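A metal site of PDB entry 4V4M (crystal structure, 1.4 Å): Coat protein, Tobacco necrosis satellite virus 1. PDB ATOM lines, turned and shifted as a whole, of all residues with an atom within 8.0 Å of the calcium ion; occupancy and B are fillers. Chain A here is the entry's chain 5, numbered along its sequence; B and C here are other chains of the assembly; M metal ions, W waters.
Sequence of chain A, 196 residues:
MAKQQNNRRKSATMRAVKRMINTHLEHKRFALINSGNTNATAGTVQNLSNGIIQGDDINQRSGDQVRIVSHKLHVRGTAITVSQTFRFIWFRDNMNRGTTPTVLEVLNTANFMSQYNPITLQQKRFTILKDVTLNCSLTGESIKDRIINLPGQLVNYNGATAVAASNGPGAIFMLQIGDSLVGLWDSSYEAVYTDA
NZ of Lys 28 of chain A is in salt-bridge range of OD1 of Asp 195 of chain A.
The side-chain hydroxyl of Ser 62 lies within hydrogen-bond range of the side-chain amino group of Lys 28 of chain B.
The chain-end carboxylate (OXT) of Ala 196 sits at hydrogen-bond distance from the backbone NH (N) of Glu 26 of chain B.
N of Asp 64 lies within hydrogen-bond range of OE2 of Glu 26 of chain B (2.8 Å).
The side-chain carboxylate of Glu 26 of chain B sits at hydrogen-bond distance from the side-chain amide nitrogen of Gln 122 of chain C (2.9 Å).
The nearest printed residue that does not touch the calcium ion is Ala 196 (4.4 Å).
The calcium ion is bound by OD2 of Asp 195 of chain A (2.2 Å), O of Ser 62 (2.3 Å), OE1 of Glu 26 of chain B (2.3 Å), O of Gln 65 (2.4 Å), water W2 (2.4 Å) and water W1 (2.5 Å).
The calcium ion has six donor atoms within binding distance.
Water W1 lies within hydrogen-bond range of O of Asp 195 of chain A and OXT of Ala 196.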
ATOM      1  N   LYS A  28      11.511 -26.321   7.813  1.00  0.00           N
ATOM      2  CA  LYS A  28      12.151 -25.518   6.789  1.00  0.00           C
ATOM      3  C   LYS A  28      12.204 -24.061   7.254  1.00  0.00           C
ATOM      4  O   LYS A  28      11.519 -23.676   8.200  1.00  0.00           O
ATOM      5  CB  LYS A  28      11.385 -25.692   5.471  1.00  0.00           C
ATOM      6  CG  LYS A  28      11.525 -27.118   4.873  1.00  0.00           C
ATOM      7  CD  LYS A  28      10.871 -27.237   3.500  1.00  0.00           C
ATOM      8  CE  LYS A  28      11.115 -28.601   2.881  1.00  0.00           C
ATOM      9  NZ  LYS A  28      10.298 -28.807   1.643  1.00  0.00           N
ATOM     10  N   GLN A  60      12.359 -23.365   0.411  1.00  0.00           N
ATOM     11  CA  GLN A  60      11.366 -23.501  -0.649  1.00  0.00           C
ATOM     12  C   GLN A  60      10.221 -24.398  -0.179  1.00  0.00           C
ATOM     13  O   GLN A  60      10.142 -24.730   0.994  1.00  0.00           O
ATOM     14  CB  GLN A  60      12.039 -24.041  -1.918  1.00  0.00           C
ATOM     15  CG  GLN A  60      13.063 -23.028  -2.510  1.00  0.00           C
ATOM     16  CD  GLN A  60      13.850 -23.552  -3.687  1.00  0.00           C
ATOM     17  OE1 GLN A  60      14.119 -24.739  -3.794  1.00  0.00           O
ATOM     18  NE2 GLN A  60      14.245 -22.643  -4.560  1.00  0.00           N
ATOM     19  N   ARG A  61       9.329 -24.778  -1.095  1.00  0.00           N
ATOM     20  CA  ARG A  61       8.158 -25.572  -0.684  1.00  0.00           C
ATOM     21  C   ARG A  61       7.774 -26.590  -1.747  1.00  0.00           C
ATOM     22  O   ARG A  61       7.941 -26.374  -2.941  1.00  0.00           O
ATOM     23  CB  ARG A  61       6.925 -24.647  -0.398  1.00  0.00           C
ATOM     24  CG  ARG A  61       6.516 -23.805  -1.619  1.00  0.00           C
ATOM     25  CD  ARG A  61       5.350 -22.836  -1.313  1.00  0.00           C
ATOM     26  NE  ARG A  61       5.339 -21.705  -2.243  1.00  0.00           N
ATOM     27  CZ  ARG A  61       4.625 -21.657  -3.366  1.00  0.00           C
ATOM     28  NH1 ARG A  61       3.849 -22.665  -3.733  1.00  0.00           N
ATOM     29  NH2 ARG A  61       4.707 -20.595  -4.151  1.00  0.00           N
ATOM     30  N   SER A  62       7.192 -27.683  -1.271  1.00  0.00           N
ATOM     31  CA  SER A  62       6.487 -28.621  -2.125  1.00  0.00           C
ATOM     32  C   SER A  62       4.994 -28.248  -2.130  1.00  0.00           C
ATOM     33  O   SER A  62       4.391 -28.000  -1.087  1.00  0.00           O
ATOM     34  CB  SER A  62       6.684 -30.035  -1.557  1.00  0.00           C
ATOM     35  OG  SER A  62       6.116 -31.012  -2.401  1.00  0.00           O
ATOM     36  N   GLY A  63       4.398 -28.160  -3.306  1.00  0.00           N
ATOM     37  CA  GLY A  63       2.961 -27.849  -3.399  1.00  0.00           C
ATOM     38  C   GLY A  63       2.628 -26.396  -3.107  1.00  0.00           C
ATOM     39  O   GLY A  63       3.473 -25.520  -3.214  1.00  0.00           O
ATOM     40  N   ASP A  64       1.365 -26.141  -2.744  1.00  0.00           N
ATOM     41  CA  ASP A  64       0.888 -24.783  -2.569  1.00  0.00           C
ATOM     42  C   ASP A  64       0.447 -24.491  -1.139  1.00  0.00           C
ATOM     43  O   ASP A  64      -0.297 -23.549  -0.916  1.00  0.00           O
ATOM     44  CB  ASP A  64      -0.273 -24.514  -3.532  1.00  0.00           C
ATOM     45  CG  ASP A  64       0.199 -24.208  -4.944  1.00  0.00           C
ATOM     46  OD1 ASP A  64       1.360 -23.782  -5.106  1.00  0.00           O
ATOM     47  OD2 ASP A  64      -0.589 -24.389  -5.900  1.00  0.00           O
ATOM     48  N   GLN A  65       0.886 -25.292  -0.175  1.00  0.00           N
ATOM     49  CA  GLN A  65       0.655 -24.985   1.236  1.00  0.00           C
ATOM     50  C   GLN A  65       1.937 -25.171   2.022  1.00  0.00           C
ATOM     51  O   GLN A  65       2.712 -26.086   1.750  1.00  0.00           O
ATOM     52  CB  GLN A  65      -0.407 -25.920   1.832  1.00  0.00           C
ATOM     53  CG  GLN A  65      -1.821 -25.729   1.317  1.00  0.00           C
ATOM     54  CD  GLN A  65      -2.844 -26.451   2.185  1.00  0.00           C
ATOM     55  OE1 GLN A  65      -2.549 -27.476   2.795  1.00  0.00           O
ATOM     56  NE2 GLN A  65      -4.037 -25.921   2.241  1.00  0.00           N
ATOM     57  N   VAL A  66       2.161 -24.284   3.000  1.00  0.00           N
ATOM     58  CA  VAL A  66       3.101 -24.523   4.090  1.00  0.00           C
ATOM     59  C   VAL A  66       2.370 -24.168   5.392  1.00  0.00           C
ATOM     60  O   VAL A  66       1.296 -23.539   5.366  1.00  0.00           O
ATOM     61  CB  VAL A  66       4.428 -23.704   3.961  1.00  0.00           C
ATOM     62  CG1 VAL A  66       5.159 -24.028   2.645  1.00  0.00           C
ATOM     63  CG2 VAL A  66       4.174 -22.199   4.129  1.00  0.00           C
ATOM     64  N   ARG A  67       2.934 -24.572   6.532  1.00  0.00           N
ATOM     65  CA  ARG A  67       2.392 -24.150   7.816  1.00  0.00           C
ATOM     66  C   ARG A  67       3.474 -23.428   8.608  1.00  0.00           C
ATOM     67  O   ARG A  67       4.469 -24.039   8.994  1.00  0.00           O
ATOM     68  CB  ARG A  67       1.855 -25.345   8.614  1.00  0.00           C
ATOM     69  CG  ARG A  67       1.332 -24.934  10.006  1.00  0.00           C
ATOM     70  CD  ARG A  67       0.799 -26.129  10.791  1.00  0.00           C
ATOM     71  NE  ARG A  67      -0.519 -26.542  10.332  1.00  0.00           N
ATOM     72  CZ  ARG A  67      -1.598 -25.773  10.380  1.00  0.00           C
ATOM     73  NH1 ARG A  67      -1.516 -24.538  10.850  1.00  0.00           N
ATOM     74  NH2 ARG A  67      -2.773 -26.228   9.948  1.00  0.00           N
ATOM     75  N   LEU A 154      -1.327 -21.561   8.723  1.00  0.00           N
ATOM     76  CA  LEU A 154      -1.308 -22.011   7.358  1.00  0.00           C
ATOM     77  C   LEU A 154      -1.093 -20.866   6.355  1.00  0.00           C
ATOM     78  O   LEU A 154      -1.627 -19.771   6.509  1.00  0.00           O
ATOM     79  CB  LEU A 154      -2.650 -22.690   7.051  1.00  0.00           C
ATOM     80  CG  LEU A 154      -2.912 -23.297   5.668  1.00  0.00           C
ATOM     81  CD1 LEU A 154      -1.893 -24.370   5.362  1.00  0.00           C
ATOM     82  CD2 LEU A 154      -4.334 -23.879   5.633  1.00  0.00           C
ATOM     83  N   VAL A 155      -0.311 -21.161   5.320  1.00  0.00           N
ATOM     84  CA  VAL A 155      -0.199 -20.281   4.157  1.00  0.00           C
ATOM     85  C   VAL A 155      -0.535 -21.092   2.889  1.00  0.00           C
ATOM     86  O   VAL A 155       0.090 -22.130   2.608  1.00  0.00           O
ATOM     87  CB  VAL A 155       1.225 -19.695   4.008  1.00  0.00           C
ATOM     88  CG1 VAL A 155       1.266 -18.701   2.841  1.00  0.00           C
ATOM     89  CG2 VAL A 155       1.672 -19.015   5.314  1.00  0.00           C
ATOM     90  N   TYR A 157      -0.830 -20.916  -1.344  1.00  0.00           N
ATOM     91  CA  TYR A 157      -0.334 -20.186  -2.507  1.00  0.00           C
ATOM     92  C   TYR A 157      -1.223 -20.423  -3.737  1.00  0.00           C
ATOM     93  O   TYR A 157      -1.927 -21.449  -3.818  1.00  0.00           O
ATOM     94  CB  TYR A 157       1.108 -20.606  -2.834  1.00  0.00           C
ATOM     95  CG  TYR A 157       2.097 -20.137  -1.786  1.00  0.00           C
ATOM     96  CD1 TYR A 157       2.255 -20.845  -0.593  1.00  0.00           C
ATOM     97  CD2 TYR A 157       2.870 -18.976  -1.962  1.00  0.00           C
ATOM     98  CE1 TYR A 157       3.135 -20.424   0.394  1.00  0.00           C
ATOM     99  CE2 TYR A 157       3.772 -18.545  -0.969  1.00  0.00           C
ATOM    100  CZ  TYR A 157       3.888 -19.280   0.204  1.00  0.00           C
ATOM    101  OH  TYR A 157       4.747 -18.899   1.199  1.00  0.00           O
ATOM    102  N   TYR A 193       8.815 -23.033   9.046  1.00  0.00           N
ATOM    103  CA  TYR A 193       7.556 -23.666   8.593  1.00  0.00           C
ATOM    104  C   TYR A 193       7.705 -25.152   8.328  1.00  0.00           C
ATOM    105  O   TYR A 193       8.781 -25.617   7.951  1.00  0.00           O
ATOM    106  CB  TYR A 193       7.047 -22.955   7.334  1.00  0.00           C
ATOM    107  CG  TYR A 193       8.013 -22.964   6.158  1.00  0.00           C
ATOM    108  CD1 TYR A 193       9.038 -22.020   6.060  1.00  0.00           C
ATOM    109  CD2 TYR A 193       7.898 -23.897   5.138  1.00  0.00           C
ATOM    110  CE1 TYR A 193       9.927 -22.015   4.972  1.00  0.00           C
ATOM    111  CE2 TYR A 193       8.782 -23.889   4.034  1.00  0.00           C
ATOM    112  CZ  TYR A 193       9.805 -22.948   3.979  1.00  0.00           C
ATOM    113  OH  TYR A 193      10.699 -22.931   2.923  1.00  0.00           O
ATOM    114  N   THR A 194       6.611 -25.892   8.475  1.00  0.00           N
ATOM    115  CA  THR A 194       6.607 -27.280   8.034  1.00  0.00           C
ATOM    116  C   THR A 194       5.950 -27.342   6.676  1.00  0.00           C
ATOM    117  O   THR A 194       5.235 -26.428   6.266  1.00  0.00           O
ATOM    118  CB  THR A 194       5.874 -28.200   9.007  1.00  0.00           C
ATOM    119  OG1 THR A 194       4.499 -27.792   9.132  1.00  0.00           O
ATOM    120  CG2 THR A 194       6.576 -28.161  10.378  1.00  0.00           C
ATOM    121  N   ASP A 195       6.235 -28.426   5.962  1.00  0.00           N
ATOM    122  CA  ASP A 195       5.877 -28.532   4.566  1.00  0.00           C
ATOM    123  C   ASP A 195       5.539 -29.983   4.247  1.00  0.00           C
ATOM    124  O   ASP A 195       6.037 -30.578   3.286  1.00  0.00           O
ATOM    125  CB  ASP A 195       7.039 -28.008   3.706  1.00  0.00           C
ATOM    126  CG  ASP A 195       6.714 -27.964   2.226  1.00  0.00           C
ATOM    127  OD1 ASP A 195       7.654 -28.138   1.423  1.00  0.00           O
ATOM    128  OD2 ASP A 195       5.526 -27.765   1.851  1.00  0.00           O
ATOM    129  N   ALA A 196       4.691 -30.556   5.088  1.00  0.00           N
ATOM    130  CA  ALA A 196       4.352 -31.978   4.975  1.00  0.00           C
ATOM    131  C   ALA A 196       3.100 -32.227   4.147  1.00  0.00           C
ATOM    132  O   ALA A 196       2.859 -33.368   3.780  1.00  0.00           O
ATOM    133  CB  ALA A 196       4.191 -32.596   6.341  1.00  0.00           C
ATOM    134  OXT ALA A 196       2.318 -31.327   3.813  1.00  0.00           O
ATOM    135  N   HIS B  24      -1.879 -31.397   9.523  1.00  0.00           N
ATOM    136  CA  HIS B  24      -0.511 -30.981   9.267  1.00  0.00           C
ATOM    137  C   HIS B  24      -0.020 -31.306   7.859  1.00  0.00           C
ATOM    138  O   HIS B  24       1.068 -30.901   7.462  1.00  0.00           O
ATOM    139  CB  HIS B  24       0.435 -31.583  10.302  1.00  0.00           C
ATOM    140  CG  HIS B  24       0.333 -30.943  11.645  1.00  0.00           C
ATOM    141  ND1 HIS B  24       1.255 -30.019  12.106  1.00  0.00           N
ATOM    142  CD2 HIS B  24      -0.593 -31.072  12.625  1.00  0.00           C
ATOM    143  CE1 HIS B  24       0.893 -29.609  13.310  1.00  0.00           C
ATOM    144  NE2 HIS B  24      -0.220 -30.229  13.645  1.00  0.00           N
ATOM    145  N   LEU B  25      -0.837 -32.035   7.100  1.00  0.00           N
ATOM    146  CA  LEU B  25      -0.436 -32.522   5.781  1.00  0.00           C
ATOM    147  C   LEU B  25      -1.163 -31.802   4.657  1.00  0.00           C
ATOM    148  O   LEU B  25      -2.401 -31.714   4.671  1.00  0.00           O
ATOM    149  CB  LEU B  25      -0.755 -34.026   5.651  1.00  0.00           C
ATOM    150  CG  LEU B  25      -0.229 -34.959   6.735  1.00  0.00           C
ATOM    151  CD1 LEU B  25      -0.405 -36.403   6.301  1.00  0.00           C
ATOM    152  CD2 LEU B  25       1.243 -34.672   7.053  1.00  0.00           C
ATOM    153  N   GLU B  26      -0.416 -31.323   3.660  1.00  0.00           N
ATOM    154  CA  GLU B  26      -1.051 -30.711   2.509  1.00  0.00           C
ATOM    155  C   GLU B  26      -1.887 -31.746   1.748  1.00  0.00           C
ATOM    156  O   GLU B  26      -1.419 -32.839   1.420  1.00  0.00           O
ATOM    157  CB  GLU B  26      -0.032 -30.069   1.565  1.00  0.00           C
ATOM    158  CG  GLU B  26      -0.671 -29.386   0.333  1.00  0.00           C
ATOM    159  CD  GLU B  26       0.322 -28.607  -0.536  1.00  0.00           C
ATOM    160  OE1 GLU B  26       1.449 -28.310  -0.083  1.00  0.00           O
ATOM    161  OE2 GLU B  26      -0.033 -28.312  -1.704  1.00  0.00           O
ATOM    162  N   HIS B  27      -3.127 -31.373   1.493  1.00  0.00           N
ATOM    163  CA  HIS B  27      -4.000 -32.180   0.650  1.00  0.00           C
ATOM    164  C   HIS B  27      -3.834 -31.674  -0.775  1.00  0.00           C
ATOM    165  O   HIS B  27      -4.502 -30.716  -1.208  1.00  0.00           O
ATOM    166  CB  HIS B  27      -5.439 -32.134   1.180  1.00  0.00           C
ATOM    167  CG  HIS B  27      -5.569 -32.813   2.509  1.00  0.00           C
ATOM    168  ND1 HIS B  27      -6.508 -33.783   2.765  1.00  0.00           N
ATOM    169  CD2 HIS B  27      -4.833 -32.699   3.633  1.00  0.00           C
ATOM    170  CE1 HIS B  27      -6.361 -34.218   4.003  1.00  0.00           C
ATOM    171  NE2 HIS B  27      -5.353 -33.575   4.559  1.00  0.00           N
ATOM    172  N   LYS B  28      -2.897 -32.294  -1.475  1.00  0.00           N
ATOM    173  CA  LYS B  28      -2.661 -31.983  -2.875  1.00  0.00           C
ATOM    174  C   LYS B  28      -3.847 -32.467  -3.694  1.00  0.00           C
ATOM    175  O   LYS B  28      -4.687 -33.207  -3.177  1.00  0.00           O
ATOM    176  CB  LYS B  28      -1.339 -32.580  -3.351  1.00  0.00           C
ATOM    177  CG  LYS B  28      -0.115 -31.956  -2.673  1.00  0.00           C
ATOM    178  CD  LYS B  28       1.206 -32.505  -3.222  1.00  0.00           C
ATOM    179  CE  LYS B  28       2.386 -31.806  -2.564  1.00  0.00           C
ATOM    180  NZ  LYS B  28       3.693 -32.404  -2.985  1.00  0.00           N
ATOM    181  N   ASP B  56       7.017 -30.498  -8.032  1.00  0.00           N
ATOM    182  CA  ASP B  56       6.779 -29.677  -6.860  1.00  0.00           C
ATOM    183  C   ASP B  56       5.422 -28.998  -6.865  1.00  0.00           C
ATOM    184  O   ASP B  56       5.110 -28.262  -5.936  1.00  0.00           O
ATOM    185  CB  ASP B  56       7.868 -28.594  -6.753  1.00  0.00           C
ATOM    186  CG  ASP B  56       9.266 -29.175  -6.712  1.00  0.00           C
ATOM    187  OD1 ASP B  56       9.427 -30.304  -6.225  1.00  0.00           O
ATOM    188  OD2 ASP B  56      10.197 -28.485  -7.174  1.00  0.00           O
ATOM    189  N   ASP B 195       0.933 -36.400   0.672  1.00  0.00           N
ATOM    190  CA  ASP B 195       2.184 -36.713   0.018  1.00  0.00           C
ATOM    191  C   ASP B 195       3.315 -36.431   0.995  1.00  0.00           C
ATOM    192  O   ASP B 195       4.288 -35.744   0.679  1.00  0.00           O
ATOM    193  CB  ASP B 195       2.343 -35.829  -1.227  1.00  0.00           C
ATOM    194  CG  ASP B 195       3.581 -36.152  -2.026  1.00  0.00           C
ATOM    195  OD1 ASP B 195       4.142 -35.238  -2.666  1.00  0.00           O
ATOM    196  OD2 ASP B 195       4.005 -37.323  -2.036  1.00  0.00           O
ATOM    197  N   GLN C 122      -8.469 -26.392  -2.802  1.00  0.00           N
ATOM    198  CA  GLN C 122      -7.529 -26.694  -1.720  1.00  0.00           C
ATOM    199  C   GLN C 122      -7.558 -25.602  -0.644  1.00  0.00           C
ATOM    200  O   GLN C 122      -7.619 -25.890   0.572  1.00  0.00           O
ATOM    201  CB  GLN C 122      -6.097 -26.848  -2.231  1.00  0.00           C
ATOM    202  CG  GLN C 122      -5.047 -27.029  -1.115  1.00  0.00           C
ATOM    203  CD  GLN C 122      -3.601 -26.969  -1.633  1.00  0.00           C
ATOM    204  OE1 GLN C 122      -3.093 -25.893  -1.977  1.00  0.00           O
ATOM    205  NE2 GLN C 122      -2.938 -28.109  -1.676  1.00  0.00           N
HETATM  206 CA    CA M   1       3.492 -28.180   1.005  1.00  0.00          CA
HETATM  207  O   HOH W   1       4.039 -30.580   1.034  1.00  0.00           O
HETATM  208  O   HOH W   2       2.639 -28.841   3.155  1.00  0.00           O
